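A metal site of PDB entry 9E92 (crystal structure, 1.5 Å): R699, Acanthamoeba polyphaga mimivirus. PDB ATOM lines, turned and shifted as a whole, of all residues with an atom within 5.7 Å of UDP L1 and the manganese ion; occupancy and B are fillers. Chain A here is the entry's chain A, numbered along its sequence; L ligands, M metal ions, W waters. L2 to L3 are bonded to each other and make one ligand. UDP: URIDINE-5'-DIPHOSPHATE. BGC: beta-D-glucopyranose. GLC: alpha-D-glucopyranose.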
ATOM      1  N   GLY A  17     -13.761  -0.977  -9.732  1.00  0.00           N
ATOM      2  CA  GLY A  17     -12.807  -0.246 -10.539  1.00  0.00           C
ATOM      3  C   GLY A  17     -11.789  -1.176 -11.156  1.00  0.00           C
ATOM      4  O   GLY A  17     -11.133  -1.950 -10.407  1.00  0.00           O
ATOM      5  N   ILE A  18     -11.601  -1.111 -12.470  1.00  0.00           N
ATOM      6  CA  ILE A  18     -10.651  -1.974 -13.166  1.00  0.00           C
ATOM      7  C   ILE A  18      -9.222  -1.428 -13.023  1.00  0.00           C
ATOM      8  O   ILE A  18      -8.944  -0.277 -13.409  1.00  0.00           O
ATOM      9  CB  ILE A  18     -10.938  -2.123 -14.663  1.00  0.00           C
ATOM     10  CG1 ILE A  18     -12.386  -2.475 -14.942  1.00  0.00           C
ATOM     11  CG2 ILE A  18      -9.962  -3.088 -15.311  1.00  0.00           C
ATOM     12  CD1 ILE A  18     -12.848  -3.755 -14.290  1.00  0.00           C
ATOM     13  N   GLY A  19      -8.339  -2.205 -12.373  1.00  0.00           N
ATOM     14  CA  GLY A  19      -6.968  -1.790 -12.095  1.00  0.00           C
ATOM     15  C   GLY A  19      -6.011  -2.992 -12.185  1.00  0.00           C
ATOM     16  O   GLY A  19      -5.471  -3.459 -11.158  1.00  0.00           O
ATOM     17  N   ILE A  20      -5.814  -3.408 -13.437  1.00  0.00           N
ATOM     18  CA  ILE A  20      -4.992  -4.562 -13.764  1.00  0.00           C
ATOM     19  C   ILE A  20      -3.544  -4.100 -13.892  1.00  0.00           C
ATOM     20  O   ILE A  20      -3.149  -3.522 -14.900  1.00  0.00           O
ATOM     21  CB  ILE A  20      -5.502  -5.197 -15.054  1.00  0.00           C
ATOM     22  CG1 ILE A  20      -6.950  -5.660 -14.950  1.00  0.00           C
ATOM     23  CG2 ILE A  20      -4.613  -6.379 -15.434  1.00  0.00           C
ATOM     24  CD1 ILE A  20      -7.645  -5.834 -16.293  1.00  0.00           C
ATOM     25  N   SER A  21      -2.778  -4.467 -12.862  1.00  0.00           N
ATOM     26  CA  SER A  21      -1.361  -4.116 -12.774  1.00  0.00           C
ATOM     27  C   SER A  21      -0.720  -4.925 -11.648  1.00  0.00           C
ATOM     28  O   SER A  21      -1.300  -5.082 -10.586  1.00  0.00           O
ATOM     29  CB  SER A  21      -1.256  -2.605 -12.479  1.00  0.00           C
ATOM     30  OG  SER A  21       0.076  -2.153 -12.725  1.00  0.00           O
ATOM     31  N   VAL A  45     -10.506  -4.423  -9.352  1.00  0.00           N
ATOM     32  CA  VAL A  45     -10.490  -5.683 -10.108  1.00  0.00           C
ATOM     33  C   VAL A  45      -9.136  -5.818 -10.799  1.00  0.00           C
ATOM     34  O   VAL A  45      -8.704  -4.951 -11.557  1.00  0.00           O
ATOM     35  CB  VAL A  45     -11.648  -5.671 -11.139  1.00  0.00           C
ATOM     36  CG1 VAL A  45     -11.560  -6.822 -12.156  1.00  0.00           C
ATOM     37  CG2 VAL A  45     -12.985  -5.667 -10.383  1.00  0.00           C
ATOM     38  N   TRP A  51      -1.200  -6.411 -17.312  1.00  0.00           N
ATOM     39  CA  TRP A  51      -2.077  -5.995 -18.405  1.00  0.00           C
ATOM     40  C   TRP A  51      -1.682  -6.653 -19.729  1.00  0.00           C
ATOM     41  O   TRP A  51      -0.498  -6.615 -20.113  1.00  0.00           O
ATOM     42  CB  TRP A  51      -2.042  -4.469 -18.547  1.00  0.00           C
ATOM     43  CG  TRP A  51      -2.785  -3.874 -19.707  1.00  0.00           C
ATOM     44  CD1 TRP A  51      -2.240  -3.345 -20.833  1.00  0.00           C
ATOM     45  CD2 TRP A  51      -4.207  -3.635 -19.824  1.00  0.00           C
ATOM     46  NE1 TRP A  51      -3.191  -2.824 -21.654  1.00  0.00           N
ATOM     47  CE2 TRP A  51      -4.420  -2.954 -21.051  1.00  0.00           C
ATOM     48  CE3 TRP A  51      -5.306  -3.899 -19.005  1.00  0.00           C
ATOM     49  CZ2 TRP A  51      -5.687  -2.532 -21.476  1.00  0.00           C
ATOM     50  CZ3 TRP A  51      -6.564  -3.505 -19.437  1.00  0.00           C
ATOM     51  CH2 TRP A  51      -6.736  -2.826 -20.636  1.00  0.00           C
ATOM     52  N   LEU A  56      -3.969   1.240 -25.568  1.00  0.00           N
ATOM     53  CA  LEU A  56      -5.245   1.885 -25.840  1.00  0.00           C
ATOM     54  C   LEU A  56      -5.077   3.348 -26.283  1.00  0.00           C
ATOM     55  O   LEU A  56      -6.025   3.957 -26.793  1.00  0.00           O
ATOM     56  CB  LEU A  56      -6.208   1.769 -24.663  1.00  0.00           C
ATOM     57  CG  LEU A  56      -6.530   0.375 -24.139  1.00  0.00           C
ATOM     58  CD1 LEU A  56      -7.550   0.435 -23.015  1.00  0.00           C
ATOM     59  CD2 LEU A  56      -7.019  -0.503 -25.320  1.00  0.00           C
ATOM     60  N   LYS A  65     -10.335  -6.365 -19.691  1.00  0.00           N
ATOM     61  CA  LYS A  65     -11.146  -5.802 -18.637  1.00  0.00           C
ATOM     62  C   LYS A  65     -12.430  -6.641 -18.417  1.00  0.00           C
ATOM     63  O   LYS A  65     -12.802  -6.877 -17.276  1.00  0.00           O
ATOM     64  CB  LYS A  65     -11.528  -4.356 -19.023  1.00  0.00           C
ATOM     65  CG  LYS A  65     -10.401  -3.372 -19.184  1.00  0.00           C
ATOM     66  CD  LYS A  65     -10.816  -2.112 -19.957  1.00  0.00           C
ATOM     67  CE  LYS A  65     -11.872  -1.342 -19.303  1.00  0.00           C
ATOM     68  NZ  LYS A  65     -12.586  -0.291 -20.076  1.00  0.00           N
ATOM     69  N   CYS A  85     -16.076   0.663 -13.669  1.00  0.00           N
ATOM     70  CA  CYS A  85     -15.472   1.841 -14.291  1.00  0.00           C
ATOM     71  C   CYS A  85     -13.962   1.712 -14.435  1.00  0.00           C
ATOM     72  O   CYS A  85     -13.267   0.957 -13.695  1.00  0.00           O
ATOM     73  CB  CYS A  85     -15.809   3.110 -13.512  1.00  0.00           C
ATOM     74  SG  CYS A  85     -15.244   3.101 -11.784  1.00  0.00           S
ATOM     75  N   ASP A  86     -13.456   2.476 -15.391  1.00  0.00           N
ATOM     76  CA  ASP A  86     -12.041   2.826 -15.561  1.00  0.00           C
ATOM     77  C   ASP A  86     -11.518   3.448 -14.263  1.00  0.00           C
ATOM     78  O   ASP A  86     -12.314   4.053 -13.524  1.00  0.00           O
ATOM     79  CB  ASP A  86     -11.784   3.752 -16.741  1.00  0.00           C
ATOM     80  CG  ASP A  86     -11.905   3.170 -18.137  1.00  0.00           C
ATOM     81  OD1 ASP A  86     -12.335   1.946 -18.189  1.00  0.00           O
ATOM     82  OD2 ASP A  86     -11.520   3.824 -19.183  1.00  0.00           O
ATOM     83  N   THR A  87     -10.190   3.272 -13.976  1.00  0.00           N
ATOM     84  CA  THR A  87      -9.587   3.894 -12.805  1.00  0.00           C
ATOM     85  C   THR A  87      -8.400   4.803 -13.124  1.00  0.00           C
ATOM     86  O   THR A  87      -8.070   5.631 -12.264  1.00  0.00           O
ATOM     87  CB  THR A  87      -9.157   2.915 -11.714  1.00  0.00           C
ATOM     88  OG1 THR A  87      -8.113   2.105 -12.244  1.00  0.00           O
ATOM     89  CG2 THR A  87     -10.339   2.068 -11.241  1.00  0.00           C
ATOM     90  N   TYR A  88      -7.752   4.645 -14.280  1.00  0.00           N
ATOM     91  CA  TYR A  88      -6.480   5.304 -14.506  1.00  0.00           C
ATOM     92  C   TYR A  88      -6.697   6.788 -14.788  1.00  0.00           C
ATOM     93  O   TYR A  88      -5.839   7.630 -14.499  1.00  0.00           O
ATOM     94  CB  TYR A  88      -5.679   4.667 -15.633  1.00  0.00           C
ATOM     95  CG  TYR A  88      -4.937   3.366 -15.269  1.00  0.00           C
ATOM     96  CD1 TYR A  88      -5.296   2.646 -14.148  1.00  0.00           C
ATOM     97  CD2 TYR A  88      -3.862   2.945 -16.011  1.00  0.00           C
ATOM     98  CE1 TYR A  88      -4.655   1.453 -13.799  1.00  0.00           C
ATOM     99  CE2 TYR A  88      -3.200   1.768 -15.671  1.00  0.00           C
ATOM    100  CZ  TYR A  88      -3.578   1.067 -14.563  1.00  0.00           C
ATOM    101  OH  TYR A  88      -2.899  -0.098 -14.137  1.00  0.00           O
ATOM    102  N   ASP A  89      -7.884   7.115 -15.358  1.00  0.00           N
ATOM    103  CA  ASP A  89      -8.239   8.433 -15.855  1.00  0.00           C
ATOM    104  C   ASP A  89      -9.650   8.861 -15.405  1.00  0.00           C
ATOM    105  O   ASP A  89     -10.391   9.466 -16.198  1.00  0.00           O
ATOM    106  CB  ASP A  89      -8.172   8.427 -17.391  1.00  0.00           C
ATOM    107  CG  ASP A  89      -9.055   7.378 -18.087  1.00  0.00           C
ATOM    108  OD1 ASP A  89      -9.674   6.564 -17.382  1.00  0.00           O
ATOM    109  OD2 ASP A  89      -9.155   7.480 -19.343  1.00  0.00           O
ATOM    110  N   ASN A 141     -19.852   4.819 -24.396  1.00  0.00           N
ATOM    111  CA  ASN A 141     -18.502   4.718 -23.846  1.00  0.00           C
ATOM    112  C   ASN A 141     -18.504   3.658 -22.741  1.00  0.00           C
ATOM    113  O   ASN A 141     -19.329   3.673 -21.801  1.00  0.00           O
ATOM    114  CB  ASN A 141     -18.003   6.079 -23.300  1.00  0.00           C
ATOM    115  CG  ASN A 141     -16.605   5.970 -22.717  1.00  0.00           C
ATOM    116  OD1 ASN A 141     -16.504   5.580 -21.551  1.00  0.00           O
ATOM    117  ND2 ASN A 141     -15.586   6.276 -23.492  1.00  0.00           N
ATOM    118  N   GLY A 143     -16.168   2.971 -20.498  1.00  0.00           N
ATOM    119  CA  GLY A 143     -15.353   3.290 -19.344  1.00  0.00           C
ATOM    120  C   GLY A 143     -16.114   3.524 -18.043  1.00  0.00           C
ATOM    121  O   GLY A 143     -15.515   3.657 -16.964  1.00  0.00           O
ATOM    122  N   HIS A 219     -14.514  11.359 -16.235  1.00  0.00           N
ATOM    123  CA  HIS A 219     -13.681  10.451 -17.002  1.00  0.00           C
ATOM    124  C   HIS A 219     -12.916  11.230 -18.083  1.00  0.00           C
ATOM    125  O   HIS A 219     -13.475  11.666 -19.101  1.00  0.00           O
ATOM    126  CB  HIS A 219     -14.587   9.365 -17.619  1.00  0.00           C
ATOM    127  CG  HIS A 219     -13.848   8.324 -18.386  1.00  0.00           C
ATOM    128  ND1 HIS A 219     -14.470   7.459 -19.269  1.00  0.00           N
ATOM    129  CD2 HIS A 219     -12.480   7.946 -18.388  1.00  0.00           C
ATOM    130  CE1 HIS A 219     -13.553   6.598 -19.744  1.00  0.00           C
ATOM    131  NE2 HIS A 219     -12.319   6.866 -19.253  1.00  0.00           N
ATOM    132  N   GLY A 220     -11.595  11.336 -17.894  1.00  0.00           N
ATOM    133  CA  GLY A 220     -10.685  11.900 -18.876  1.00  0.00           C
ATOM    134  C   GLY A 220     -10.304  10.906 -19.936  1.00  0.00           C
ATOM    135  O   GLY A 220      -9.127  10.558 -20.044  1.00  0.00           O
ATOM    136  N   ASN A 221     -11.279  10.540 -20.740  1.00  0.00           N
ATOM    137  CA  ASN A 221     -11.082   9.489 -21.737  1.00  0.00           C
ATOM    138  C   ASN A 221     -10.172   9.993 -22.855  1.00  0.00           C
ATOM    139  O   ASN A 221     -10.103  11.182 -23.213  1.00  0.00           O
ATOM    140  CB  ASN A 221     -12.404   8.946 -22.256  1.00  0.00           C
ATOM    141  CG  ASN A 221     -13.234   9.940 -23.027  1.00  0.00           C
ATOM    142  OD1 ASN A 221     -13.519  11.052 -22.514  1.00  0.00           O
ATOM    143  ND2 ASN A 221     -13.594   9.654 -24.279  1.00  0.00           N
ATOM    144  N   GLY A 222      -9.359   9.074 -23.394  1.00  0.00           N
ATOM    145  CA  GLY A 222      -8.460   9.435 -24.467  1.00  0.00           C
ATOM    146  C   GLY A 222      -7.502  10.557 -24.044  1.00  0.00           C
ATOM    147  O   GLY A 222      -7.044  10.568 -22.899  1.00  0.00           O
ATOM    148  N   PRO A 223      -7.190  11.535 -24.903  1.00  0.00           N
ATOM    149  CA  PRO A 223      -6.344  12.663 -24.532  1.00  0.00           C
ATOM    150  C   PRO A 223      -6.868  13.548 -23.406  1.00  0.00           C
ATOM    151  O   PRO A 223      -6.097  14.358 -22.887  1.00  0.00           O
ATOM    152  CB  PRO A 223      -6.177  13.460 -25.855  1.00  0.00           C
ATOM    153  CG  PRO A 223      -6.506  12.420 -26.909  1.00  0.00           C
ATOM    154  CD  PRO A 223      -7.528  11.517 -26.342  1.00  0.00           C
ATOM    155  N   LYS A 225      -7.241  12.985 -20.472  1.00  0.00           N
ATOM    156  CA  LYS A 225      -6.458  12.867 -19.244  1.00  0.00           C
ATOM    157  C   LYS A 225      -5.851  14.236 -18.903  1.00  0.00           C
ATOM    158  O   LYS A 225      -5.735  14.561 -17.733  1.00  0.00           O
ATOM    159  CB  LYS A 225      -5.378  11.808 -19.388  1.00  0.00           C
ATOM    160  CG  LYS A 225      -5.873  10.404 -19.459  1.00  0.00           C
ATOM    161  CD  LYS A 225      -5.045   9.477 -20.340  1.00  0.00           C
ATOM    162  CE  LYS A 225      -5.787   8.139 -20.542  1.00  0.00           C
ATOM    163  NZ  LYS A 225      -7.112   8.313 -21.119  1.00  0.00           N
HETATM  164  N1  UDP L   1      -6.238  -0.559 -17.506  1.00  0.00           N
HETATM  165  C2  UDP L   1      -5.736  -1.381 -16.513  1.00  0.00           C
HETATM  166  N3  UDP L   1      -4.374  -1.620 -16.609  1.00  0.00           N
HETATM  167  C4  UDP L   1      -3.535  -1.150 -17.595  1.00  0.00           C
HETATM  168  C5  UDP L   1      -4.140  -0.342 -18.611  1.00  0.00           C
HETATM  169  C6  UDP L   1      -5.473  -0.101 -18.557  1.00  0.00           C
HETATM  170  O2  UDP L   1      -6.429  -1.770 -15.591  1.00  0.00           O
HETATM  171  O4  UDP L   1      -2.314  -1.417 -17.534  1.00  0.00           O
HETATM  172  C1' UDP L   1      -7.713  -0.240 -17.350  1.00  0.00           C
HETATM  173  C2' UDP L   1      -7.935   1.004 -16.458  1.00  0.00           C
HETATM  174  O2' UDP L   1      -9.134   0.926 -15.684  1.00  0.00           O
HETATM  175  C3' UDP L   1      -8.002   2.108 -17.485  1.00  0.00           C
HETATM  176  C4' UDP L   1      -8.839   1.410 -18.567  1.00  0.00           C
HETATM  177  O4' UDP L   1      -8.210   0.098 -18.611  1.00  0.00           O
HETATM  178  O3' UDP L   1      -8.569   3.293 -16.919  1.00  0.00           O
HETATM  179  C5' UDP L   1      -8.904   2.013 -19.927  1.00  0.00           C
HETATM  180  O5' UDP L   1      -7.654   2.550 -20.347  1.00  0.00           O
HETATM  181  PA  UDP L   1      -7.510   4.153 -20.238  1.00  0.00           P
HETATM  182  O1A UDP L   1      -6.058   4.469 -20.019  1.00  0.00           O
HETATM  183  O2A UDP L   1      -8.535   4.608 -19.265  1.00  0.00           O
HETATM  184  O3A UDP L   1      -7.938   4.681 -21.635  1.00  0.00           O
HETATM  185  PB  UDP L   1      -9.136   5.308 -22.438  1.00  0.00           P
HETATM  186  O1B UDP L   1      -8.532   6.487 -22.986  1.00  0.00           O
HETATM  187  O2B UDP L   1     -10.398   5.424 -21.539  1.00  0.00           O
HETATM  188  O3B UDP L   1      -9.166   4.122 -23.417  1.00  0.00           O
HETATM  189  C2  BGC L   2     -11.184   5.754 -25.652  1.00  0.00           C
HETATM  190  C3  BGC L   2     -12.402   6.365 -26.397  1.00  0.00           C
HETATM  191  C4  BGC L   2     -11.986   7.334 -27.502  1.00  0.00           C
HETATM  192  C5  BGC L   2     -10.955   6.598 -28.378  1.00  0.00           C
HETATM  193  C6  BGC L   2     -10.357   7.462 -29.447  1.00  0.00           C
HETATM  194  C1  BGC L   2     -10.218   5.070 -26.631  1.00  0.00           C
HETATM  195  O1  BGC L   2      -9.104   4.450 -25.996  1.00  0.00           O
HETATM  196  O2  BGC L   2     -11.550   4.809 -24.635  1.00  0.00           O
HETATM  197  O3  BGC L   2     -13.269   7.044 -25.484  1.00  0.00           O
HETATM  198  O4  BGC L   2     -13.134   7.753 -28.283  1.00  0.00           O
HETATM  199  O5  BGC L   2      -9.861   6.101 -27.553  1.00  0.00           O
HETATM  200  O6  BGC L   2      -9.775   8.621 -28.855  1.00  0.00           O
HETATM  201  C1  GLC L   3     -12.781   3.942 -24.660  1.00  0.00           C
HETATM  202  C2  GLC L   3     -13.081   3.666 -23.216  1.00  0.00           C
HETATM  203  C3  GLC L   3     -12.167   2.637 -22.559  1.00  0.00           C
HETATM  204  C4  GLC L   3     -12.181   1.378 -23.410  1.00  0.00           C
HETATM  205  C5  GLC L   3     -11.736   1.758 -24.832  1.00  0.00           C
HETATM  206  C6  GLC L   3     -11.723   0.550 -25.770  1.00  0.00           C
HETATM  207  O2  GLC L   3     -13.066   4.949 -22.522  1.00  0.00           O
HETATM  208  O3  GLC L   3     -12.614   2.268 -21.260  1.00  0.00           O
HETATM  209  O4  GLC L   3     -11.370   0.376 -22.835  1.00  0.00           O
HETATM  210  O5  GLC L   3     -12.602   2.731 -25.410  1.00  0.00           O
HETATM  211  O6  GLC L   3     -11.199   0.872 -27.044  1.00  0.00           O
HETATM  212 MN    MN M   1     -10.482   5.651 -19.417  1.00  0.00          MN
HETATM  213  O   HOH W   1      -0.339  -0.733 -19.257  1.00  0.00           O
HETATM  214  O   HOH W   2      -4.304   2.214 -20.558  1.00  0.00           O
HETATM  215  O   HOH W   3      -6.599   6.294 -24.789  1.00  0.00           O
HETATM  216  O   HOH W   4      -0.454  -0.571 -15.238  1.00  0.00           O
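The backbone carbonyl oxygen (O) of Ile 18 lies within hydrogen-bond range of an oxygen (O2') of UDP L1.
An oxygen (O1B) of UDP L1 lies within hydrogen-bond range of the backbone NH (N) of Gly 222 (2.7 Å).
The backbone NH (N) of Ile 20 sits at hydrogen-bond distance from an oxygen (O2) of UDP L1, at 2.8 Å.
The backbone carbonyl oxygen of Ile 20 is in hydrogen-bond range of a nitrogen (N3) of UDP L1.
NZ of Lys 225 lies within salt-bridge range of O1B of UDP L1, 3.0 Å away.
The backbone NH (N) of Tyr 88 sits at hydrogen-bond distance from an oxygen (O3') of UDP L1, 3.1 Å away.
OH of Tyr 88 is in hydrogen-bond range of N3 of UDP L1, 3.3 Å away.
N of Thr 87 is in hydrogen-bond range of O2' of UDP L1.
O3 of GLC L3 is in hydrogen-bond range of OD1 of Asp 86 (3.1 Å).
O1 of BGC L2 lies within hydrogen-bond range of O of Leu 56, 3.2 Å away.
The side-chain amino group of Lys 65 lies within hydrogen-bond range of an oxygen (O3) of GLC L3, at 2.8 Å.
ND2 of Asn 221 sits at hydrogen-bond distance from O3 of BGC L2, 2.9 Å away.
An oxygen (O2) of GLC L3 sits at hydrogen-bond distance from the side-chain amide nitrogen (ND2) of Asn 141.
O1 of BGC L2 sits at hydrogen-bond distance from O3B of UDP L1, 2.6 Å away.
The side-chain carboxylate of Asp 86 is in salt-bridge range of the side-chain amino group of Lys 65 (2.9 Å).
The side-chain amide oxygen (OD1) of Asn 221 sits close to the backbone carbonyl oxygen (O) of His 219.
The side-chain amino group (NZ) of Lys 225 lies close to the side-chain carboxylate (OD2) of Asp 89, 2.8 Å away.
O of Ile 18 lies within hydrogen-bond range of OG1 of Thr 87.
N of Ile 18 lies within hydrogen-bond range of O of Cys 85 (2.9 Å).
The backbone carbonyl oxygen of Gly 222 is in hydrogen-bond range of the side-chain amino group of Lys 225 (2.9 Å).
O of Gly 220 sits at hydrogen-bond distance from N of Lys 225, at 3.1 Å.
N of Gly 19 lies within hydrogen-bond range of O of Val 45, 2.9 Å away.
Merely in contact with UDP L1: Trp 51 (3.2 Å), Leu 56 (3.4 Å), Gly 19 (3.5 Å), Lys 65 (3.7 Å) and Asn 221 (3.9 Å).
Hydrophobic or aromatic side chains that line UDP L1: Ile 18, Ile 20, Trp 51, Leu 56, Tyr 88 and His 219.
Within 4 Å of UDP L1: Ile 18, Gly 19, Ile 20, Trp 51, Leu 56, Lys 65, Asp 86, Thr 87, Tyr 88, Asp 89, His 219, Asn 221, Gly 222 and Lys 225.
The nearest printed residue that does not touch the manganese ion is Asn 221 (4.5 Å).
The manganese ion is bound by the side-chain carboxylate (OD2) of Asp 86 (2.1 Å), an oxygen (O2B) of UDP L1 (2.1 Å), a ring nitrogen (NE2) of His 219 (2.2 Å), an oxygen (O2A) of UDP L1 (2.2 Å), the side-chain carboxylate (OD2) of Asp 89 (2.3 Å) and the side-chain carboxylate (OD1) of Asp 89 (2.4 Å).
Water W3 lies within hydrogen-bond range of an oxygen (O1B) of UDP L1, the backbone carbonyl oxygen (O) of Leu 56 and an oxygen (O1) of BGC L2.
Water W4 lies within hydrogen-bond range of OH of Tyr 88 (2.7 Å), OG of Ser 21 (3.0 Å) and O4 of UDP L1 (3.1 Å).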
